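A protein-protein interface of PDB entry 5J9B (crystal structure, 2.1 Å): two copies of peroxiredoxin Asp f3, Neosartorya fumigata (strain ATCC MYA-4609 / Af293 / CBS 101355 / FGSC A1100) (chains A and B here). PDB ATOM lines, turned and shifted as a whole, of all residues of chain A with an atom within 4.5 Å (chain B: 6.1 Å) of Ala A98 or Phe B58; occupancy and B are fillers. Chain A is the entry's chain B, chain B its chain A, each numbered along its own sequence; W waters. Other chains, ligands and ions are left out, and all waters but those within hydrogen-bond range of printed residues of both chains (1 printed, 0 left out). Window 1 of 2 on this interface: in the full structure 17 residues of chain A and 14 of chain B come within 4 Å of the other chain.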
ATOM      1  N   GLU A  28     -31.476   2.841 -10.446  1.00  0.00           N
ATOM      2  CA  GLU A  28     -30.730   2.683 -11.690  1.00  0.00           C
ATOM      3  C   GLU A  28     -29.240   2.593 -11.441  1.00  0.00           C
ATOM      4  O   GLU A  28     -28.452   3.259 -12.102  1.00  0.00           O
ATOM      5  CB  GLU A  28     -31.038   3.838 -12.645  1.00  0.00           C
ATOM      6  CG  GLU A  28     -32.431   3.770 -13.223  1.00  0.00           C
ATOM      7  CD  GLU A  28     -33.487   4.369 -12.307  1.00  0.00           C
ATOM      8  OE1 GLU A  28     -33.197   5.425 -11.687  1.00  0.00           O
ATOM      9  OE2 GLU A  28     -34.599   3.786 -12.217  1.00  0.00           O
ATOM     10  N   PHE A  58     -31.611  11.648 -19.158  1.00  0.00           N
ATOM     11  CA  PHE A  58     -32.526  12.051 -18.083  1.00  0.00           C
ATOM     12  C   PHE A  58     -33.223  13.379 -18.313  1.00  0.00           C
ATOM     13  O   PHE A  58     -33.836  13.931 -17.407  1.00  0.00           O
ATOM     14  CB  PHE A  58     -31.788  12.085 -16.743  1.00  0.00           C
ATOM     15  CG  PHE A  58     -31.520  10.726 -16.185  1.00  0.00           C
ATOM     16  CD1 PHE A  58     -32.550   9.969 -15.666  1.00  0.00           C
ATOM     17  CD2 PHE A  58     -30.246  10.190 -16.213  1.00  0.00           C
ATOM     18  CE1 PHE A  58     -32.309   8.710 -15.169  1.00  0.00           C
ATOM     19  CE2 PHE A  58     -29.996   8.937 -15.713  1.00  0.00           C
ATOM     20  CZ  PHE A  58     -31.023   8.200 -15.173  1.00  0.00           C
ATOM     21  N   TYR A  94     -21.704   5.274 -17.262  1.00  0.00           N
ATOM     22  CA  TYR A  94     -22.474   5.035 -16.037  1.00  0.00           C
ATOM     23  C   TYR A  94     -23.838   5.725 -16.070  1.00  0.00           C
ATOM     24  O   TYR A  94     -24.858   5.125 -15.726  1.00  0.00           O
ATOM     25  CB  TYR A  94     -21.692   5.498 -14.798  1.00  0.00           C
ATOM     26  CG  TYR A  94     -20.415   4.705 -14.557  1.00  0.00           C
ATOM     27  CD1 TYR A  94     -20.461   3.333 -14.367  1.00  0.00           C
ATOM     28  CD2 TYR A  94     -19.174   5.329 -14.507  1.00  0.00           C
ATOM     29  CE1 TYR A  94     -19.310   2.596 -14.159  1.00  0.00           C
ATOM     30  CE2 TYR A  94     -18.010   4.592 -14.286  1.00  0.00           C
ATOM     31  CZ  TYR A  94     -18.090   3.232 -14.107  1.00  0.00           C
ATOM     32  OH  TYR A  94     -16.946   2.496 -13.884  1.00  0.00           O
ATOM     33  N   VAL A  95     -23.856   6.992 -16.460  1.00  0.00           N
ATOM     34  CA  VAL A  95     -25.107   7.738 -16.552  1.00  0.00           C
ATOM     35  C   VAL A  95     -26.022   7.122 -17.629  1.00  0.00           C
ATOM     36  O   VAL A  95     -27.199   6.890 -17.373  1.00  0.00           O
ATOM     37  CB  VAL A  95     -24.858   9.261 -16.850  1.00  0.00           C
ATOM     38  CG1 VAL A  95     -26.172  10.003 -17.035  1.00  0.00           C
ATOM     39  CG2 VAL A  95     -24.042   9.908 -15.725  1.00  0.00           C
ATOM     40  N   MET A  96     -25.483   6.840 -18.816  1.00  0.00           N
ATOM     41  CA  MET A  96     -26.285   6.226 -19.882  1.00  0.00           C
ATOM     42  C   MET A  96     -26.918   4.883 -19.453  1.00  0.00           C
ATOM     43  O   MET A  96     -28.086   4.623 -19.728  1.00  0.00           O
ATOM     44  CB  MET A  96     -25.438   6.016 -21.146  1.00  0.00           C
ATOM     45  CG  MET A  96     -25.030   7.307 -21.852  1.00  0.00           C
ATOM     46  SD  MET A  96     -26.435   8.360 -22.272  1.00  0.00           S
ATOM     47  CE  MET A  96     -27.118   7.415 -23.662  1.00  0.00           C
ATOM     48  N   SER A  97     -26.141   4.049 -18.770  1.00  0.00           N
ATOM     49  CA  SER A  97     -26.621   2.756 -18.299  1.00  0.00           C
ATOM     50  C   SER A  97     -27.762   2.920 -17.313  1.00  0.00           C
ATOM     51  O   SER A  97     -28.766   2.204 -17.381  1.00  0.00           O
ATOM     52  CB  SER A  97     -25.483   1.959 -17.659  1.00  0.00           C
ATOM     53  OG  SER A  97     -25.984   0.787 -17.031  1.00  0.00           O
ATOM     54  N   ALA A  98     -27.615   3.873 -16.399  1.00  0.00           N
ATOM     55  CA  ALA A  98     -28.694   4.185 -15.467  1.00  0.00           C
ATOM     56  C   ALA A  98     -29.953   4.661 -16.213  1.00  0.00           C
ATOM     57  O   ALA A  98     -31.067   4.279 -15.886  1.00  0.00           O
ATOM     58  CB  ALA A  98     -28.234   5.239 -14.463  1.00  0.00           C
ATOM     59  N   TRP A  99     -29.765   5.511 -17.211  1.00  0.00           N
ATOM     60  CA  TRP A  99     -30.882   6.020 -17.993  1.00  0.00           C
ATOM     61  C   TRP A  99     -31.602   4.871 -18.710  1.00  0.00           C
ATOM     62  O   TRP A  99     -32.816   4.858 -18.792  1.00  0.00           O
ATOM     63  CB  TRP A  99     -30.403   7.060 -19.009  1.00  0.00           C
ATOM     64  CG  TRP A  99     -31.510   7.896 -19.582  1.00  0.00           C
ATOM     65  CD1 TRP A  99     -32.663   8.274 -18.952  1.00  0.00           C
ATOM     66  CD2 TRP A  99     -31.573   8.452 -20.901  1.00  0.00           C
ATOM     67  NE1 TRP A  99     -33.437   9.030 -19.793  1.00  0.00           N
ATOM     68  CE2 TRP A  99     -32.796   9.150 -20.999  1.00  0.00           C
ATOM     69  CE3 TRP A  99     -30.718   8.423 -22.010  1.00  0.00           C
ATOM     70  CZ2 TRP A  99     -33.180   9.824 -22.157  1.00  0.00           C
ATOM     71  CZ3 TRP A  99     -31.108   9.092 -23.170  1.00  0.00           C
ATOM     72  CH2 TRP A  99     -32.332   9.776 -23.230  1.00  0.00           C
ATOM     73  N   GLY A 100     -30.838   3.915 -19.228  1.00  0.00           N
ATOM     74  CA  GLY A 100     -31.406   2.706 -19.794  1.00  0.00           C
ATOM     75  C   GLY A 100     -32.356   1.968 -18.852  1.00  0.00           C
ATOM     76  O   GLY A 100     -33.494   1.649 -19.225  1.00  0.00           O
ATOM     77  N   LYS A 101     -31.890   1.683 -17.635  1.00  0.00           N
ATOM     78  CA  LYS A 101     -32.733   1.059 -16.616  1.00  0.00           C
ATOM     79  C   LYS A 101     -33.937   1.915 -16.263  1.00  0.00           C
ATOM     80  O   LYS A 101     -35.026   1.402 -16.046  1.00  0.00           O
ATOM     81  CB  LYS A 101     -31.931   0.777 -15.349  1.00  0.00           C
ATOM     82  CG  LYS A 101     -30.926  -0.330 -15.508  1.00  0.00           C
ATOM     83  CD  LYS A 101     -29.759  -0.121 -14.570  1.00  0.00           C
ATOM     84  CE  LYS A 101     -28.625  -1.048 -14.934  1.00  0.00           C
ATOM     85  NZ  LYS A 101     -27.540  -0.992 -13.932  1.00  0.00           N
ATOM     86  N   ALA A 102     -33.739   3.226 -16.188  1.00  0.00           N
ATOM     87  CA  ALA A 102     -34.838   4.122 -15.864  1.00  0.00           C
ATOM     88  C   ALA A 102     -35.883   4.095 -16.979  1.00  0.00           C
ATOM     89  O   ALA A 102     -37.060   4.340 -16.746  1.00  0.00           O
ATOM     90  CB  ALA A 102     -34.328   5.530 -15.642  1.00  0.00           C
ATOM     91  N   GLY B  56     -18.528  12.094 -10.182  1.00  0.00           N
ATOM     92  CA  GLY B  56     -19.681  11.981 -11.052  1.00  0.00           C
ATOM     93  C   GLY B  56     -20.854  11.265 -10.458  1.00  0.00           C
ATOM     94  O   GLY B  56     -20.692  10.374  -9.624  1.00  0.00           O
ATOM     95  N   ALA B  57     -22.045  11.672 -10.885  1.00  0.00           N
ATOM     96  CA  ALA B  57     -23.265  10.965 -10.531  1.00  0.00           C
ATOM     97  C   ALA B  57     -23.257   9.587 -11.177  1.00  0.00           C
ATOM     98  O   ALA B  57     -22.671   9.406 -12.252  1.00  0.00           O
ATOM     99  CB  ALA B  57     -24.514  11.763 -10.975  1.00  0.00           C
ATOM    100  N   PHE B  58     -23.918   8.642 -10.504  1.00  0.00           N
ATOM    101  CA  PHE B  58     -24.139   7.264 -10.956  1.00  0.00           C
ATOM    102  C   PHE B  58     -22.880   6.391 -11.086  1.00  0.00           C
ATOM    103  O   PHE B  58     -22.928   5.334 -11.689  1.00  0.00           O
ATOM    104  CB  PHE B  58     -24.913   7.263 -12.277  1.00  0.00           C
ATOM    105  CG  PHE B  58     -26.366   7.634 -12.119  1.00  0.00           C
ATOM    106  CD1 PHE B  58     -27.269   6.735 -11.578  1.00  0.00           C
ATOM    107  CD2 PHE B  58     -26.820   8.882 -12.490  1.00  0.00           C
ATOM    108  CE1 PHE B  58     -28.599   7.069 -11.432  1.00  0.00           C
ATOM    109  CE2 PHE B  58     -28.158   9.222 -12.341  1.00  0.00           C
ATOM    110  CZ  PHE B  58     -29.043   8.315 -11.812  1.00  0.00           C
ATOM    111  N   THR B  59     -21.769   6.806 -10.493  1.00  0.00           N
ATOM    112  CA  THR B  59     -20.638   5.886 -10.313  1.00  0.00           C
ATOM    113  C   THR B  59     -21.124   4.619  -9.590  1.00  0.00           C
ATOM    114  O   THR B  59     -22.059   4.676  -8.794  1.00  0.00           O
ATOM    115  CB  THR B  59     -19.504   6.538  -9.526  1.00  0.00           C
ATOM    116  OG1 THR B  59     -20.064   7.183  -8.378  1.00  0.00           O
ATOM    117  CG2 THR B  59     -18.795   7.572 -10.390  1.00  0.00           C
ATOM    118  N   PRO B  60     -20.510   3.464  -9.880  1.00  0.00           N
ATOM    119  CA  PRO B  60     -21.181   2.231  -9.440  1.00  0.00           C
ATOM    120  C   PRO B  60     -21.296   2.077  -7.923  1.00  0.00           C
ATOM    121  O   PRO B  60     -20.665   2.802  -7.151  1.00  0.00           O
ATOM    122  CB  PRO B  60     -20.295   1.110 -10.015  1.00  0.00           C
ATOM    123  CG  PRO B  60     -19.344   1.765 -10.946  1.00  0.00           C
ATOM    124  CD  PRO B  60     -19.224   3.197 -10.545  1.00  0.00           C
ATOM    125  N   VAL B  61     -22.122   1.119  -7.522  1.00  0.00           N
ATOM    126  CA  VAL B  61     -22.338   0.777  -6.122  1.00  0.00           C
ATOM    127  C   VAL B  61     -21.064   0.235  -5.468  1.00  0.00           C
ATOM    128  O   VAL B  61     -20.741   0.569  -4.329  1.00  0.00           O
ATOM    129  CB  VAL B  61     -23.473  -0.264  -5.996  1.00  0.00           C
ATOM    130  CG1 VAL B  61     -23.705  -0.664  -4.545  1.00  0.00           C
ATOM    131  CG2 VAL B  61     -24.757   0.273  -6.627  1.00  0.00           C
ATOM    132  N   ASN B  91     -22.249  16.868 -13.413  1.00  0.00           N
ATOM    133  CA  ASN B  91     -23.424  16.463 -14.172  1.00  0.00           C
ATOM    134  C   ASN B  91     -24.483  17.561 -14.138  1.00  0.00           C
ATOM    135  O   ASN B  91     -24.576  18.300 -13.150  1.00  0.00           O
ATOM    136  CB  ASN B  91     -24.001  15.158 -13.607  1.00  0.00           C
ATOM    137  CG  ASN B  91     -22.946  14.088 -13.409  1.00  0.00           C
ATOM    138  OD1 ASN B  91     -22.197  14.119 -12.432  1.00  0.00           O
ATOM    139  ND2 ASN B  91     -22.898  13.114 -14.325  1.00  0.00           N
ATOM    140  N   VAL B  95     -29.505  14.960 -14.326  1.00  0.00           N
ATOM    141  CA  VAL B  95     -28.810  13.757 -13.885  1.00  0.00           C
ATOM    142  C   VAL B  95     -28.652  13.772 -12.364  1.00  0.00           C
ATOM    143  O   VAL B  95     -28.864  12.760 -11.699  1.00  0.00           O
ATOM    144  CB  VAL B  95     -27.429  13.622 -14.556  1.00  0.00           C
ATOM    145  CG1 VAL B  95     -26.709  12.362 -14.071  1.00  0.00           C
ATOM    146  CG2 VAL B  95     -27.582  13.588 -16.067  1.00  0.00           C
ATOM    147  N   MET B  96     -28.293  14.923 -11.809  1.00  0.00           N
ATOM    148  CA  MET B  96     -28.135  15.030 -10.358  1.00  0.00           C
ATOM    149  C   MET B  96     -29.432  14.663  -9.645  1.00  0.00           C
ATOM    150  O   MET B  96     -29.425  13.916  -8.669  1.00  0.00           O
ATOM    151  CB  MET B  96     -27.699  16.439  -9.955  1.00  0.00           C
ATOM    152  CG  MET B  96     -26.254  16.766 -10.285  1.00  0.00           C
ATOM    153  SD  MET B  96     -25.041  15.522  -9.761  1.00  0.00           S
ATOM    154  CE  MET B  96     -25.124  15.736  -7.977  1.00  0.00           C
ATOM    155  N   ALA B  98     -32.011  12.884 -10.836  1.00  0.00           N
ATOM    156  CA  ALA B  98     -32.293  11.460 -10.993  1.00  0.00           C
ATOM    157  C   ALA B  98     -31.390  10.614 -10.077  1.00  0.00           C
ATOM    158  O   ALA B  98     -31.814   9.602  -9.538  1.00  0.00           O
ATOM    159  CB  ALA B  98     -32.128  11.051 -12.432  1.00  0.00           C
ATOM    160  N   TRP B  99     -30.149  11.040  -9.892  1.00  0.00           N
ATOM    161  CA  TRP B  99     -29.244  10.344  -8.966  1.00  0.00           C
ATOM    162  C   TRP B  99     -29.728  10.404  -7.521  1.00  0.00           C
ATOM    163  O   TRP B  99     -29.536   9.469  -6.745  1.00  0.00           O
ATOM    164  CB  TRP B  99     -27.838  10.938  -9.036  1.00  0.00           C
ATOM    165  CG  TRP B  99     -26.775  10.064  -8.432  1.00  0.00           C
ATOM    166  CD1 TRP B  99     -26.728   8.688  -8.430  1.00  0.00           C
ATOM    167  CD2 TRP B  99     -25.582  10.506  -7.767  1.00  0.00           C
ATOM    168  NE1 TRP B  99     -25.577   8.256  -7.800  1.00  0.00           N
ATOM    169  CE2 TRP B  99     -24.863   9.353  -7.379  1.00  0.00           C
ATOM    170  CE3 TRP B  99     -25.055  11.765  -7.461  1.00  0.00           C
ATOM    171  CZ2 TRP B  99     -23.648   9.428  -6.695  1.00  0.00           C
ATOM    172  CZ3 TRP B  99     -23.844  11.839  -6.783  1.00  0.00           C
ATOM    173  CH2 TRP B  99     -23.158  10.679  -6.405  1.00  0.00           C
ATOM    174  N   GLY B 100     -30.326  11.526  -7.156  1.00  0.00           N
ATOM    175  CA  GLY B 100     -30.891  11.673  -5.825  1.00  0.00           C
ATOM    176  C   GLY B 100     -32.038  10.707  -5.623  1.00  0.00           C
ATOM    177  O   GLY B 100     -32.155  10.070  -4.575  1.00  0.00           O
ATOM    178  N   ALA B 102     -32.432   7.877  -7.298  1.00  0.00           N
ATOM    179  CA  ALA B 102     -31.806   6.559  -7.263  1.00  0.00           C
ATOM    180  C   ALA B 102     -31.198   6.254  -5.894  1.00  0.00           C
ATOM    181  O   ALA B 102     -31.120   5.098  -5.497  1.00  0.00           O
ATOM    182  CB  ALA B 102     -30.739   6.445  -8.348  1.00  0.00           C
HETATM  183  O   HOH W   1     -25.062   3.486 -13.379  1.00  0.00           O
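Phe B58 touches its own counterpart, Phe A58.
Phe A58 touches Ala B98, and with the chains exchanged Ala A98 touches Phe B58.
Val A95 touches its own counterpart, Val B95.
Of the 9 pairs that touch across the chains among the printed residues, 4 have their exchanged pair printed and touching as well.
N of Ala B57 lies within hydrogen-bond range of OD1 of Asn B91, 2.9 Å away.
Water W1 lies within hydrogen-bond range of O of Tyr A94 (2.9 Å) and O of Phe B58 (3.3 Å).
Of the printed residues of chain B, Glu A28 touches Phe B58 (3.7 Å).
Printed residues of chain B within 4 Å of Val A95: Ala B57 (3.8 Å), Asn B91 (3.7 Å) and Val B95 (3.8 Å).
Of the printed residues of chain A, Pro B60 touches Tyr A94.
Of the printed residues of chain A, Asn B91 touches Val A95.
The nearest printed residue of chain A that does not touch Val B95 is Phe A58 (4.3 Å).
Among the printed residues, pairs that only touch across the chains: Glu A28 with Phe B58 (3.7 Å), Phe A58 with Phe B58 (3.9 Å), Phe A58 with Ala B98 (3.4 Å), Tyr A94 with Phe B58 (3.3 Å), Tyr A94 with Pro B60 (3.3 Å), Val A95 with Ala B57 (3.8 Å), Val A95 with Asn B91 (3.7 Å), Val A95 with Val B95 (3.8 Å) and Ala A98 with Phe B58 (3.4 Å).
Of the 11 printed residues of chain A, 5 touch a printed residue of chain B.
Hydrophobic or aromatic side chains of chain A that line the printed part of chain B: Phe A58, Tyr A94, Val A95 and Ala A98.
Of the 13 printed residues of chain B, 6 touch a printed residue of chain A.
Along chain B the printed residues that touch a printed residue of chain A span positions 57 to 98.
Among the printed residues, 9 pairs touch across the chains.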
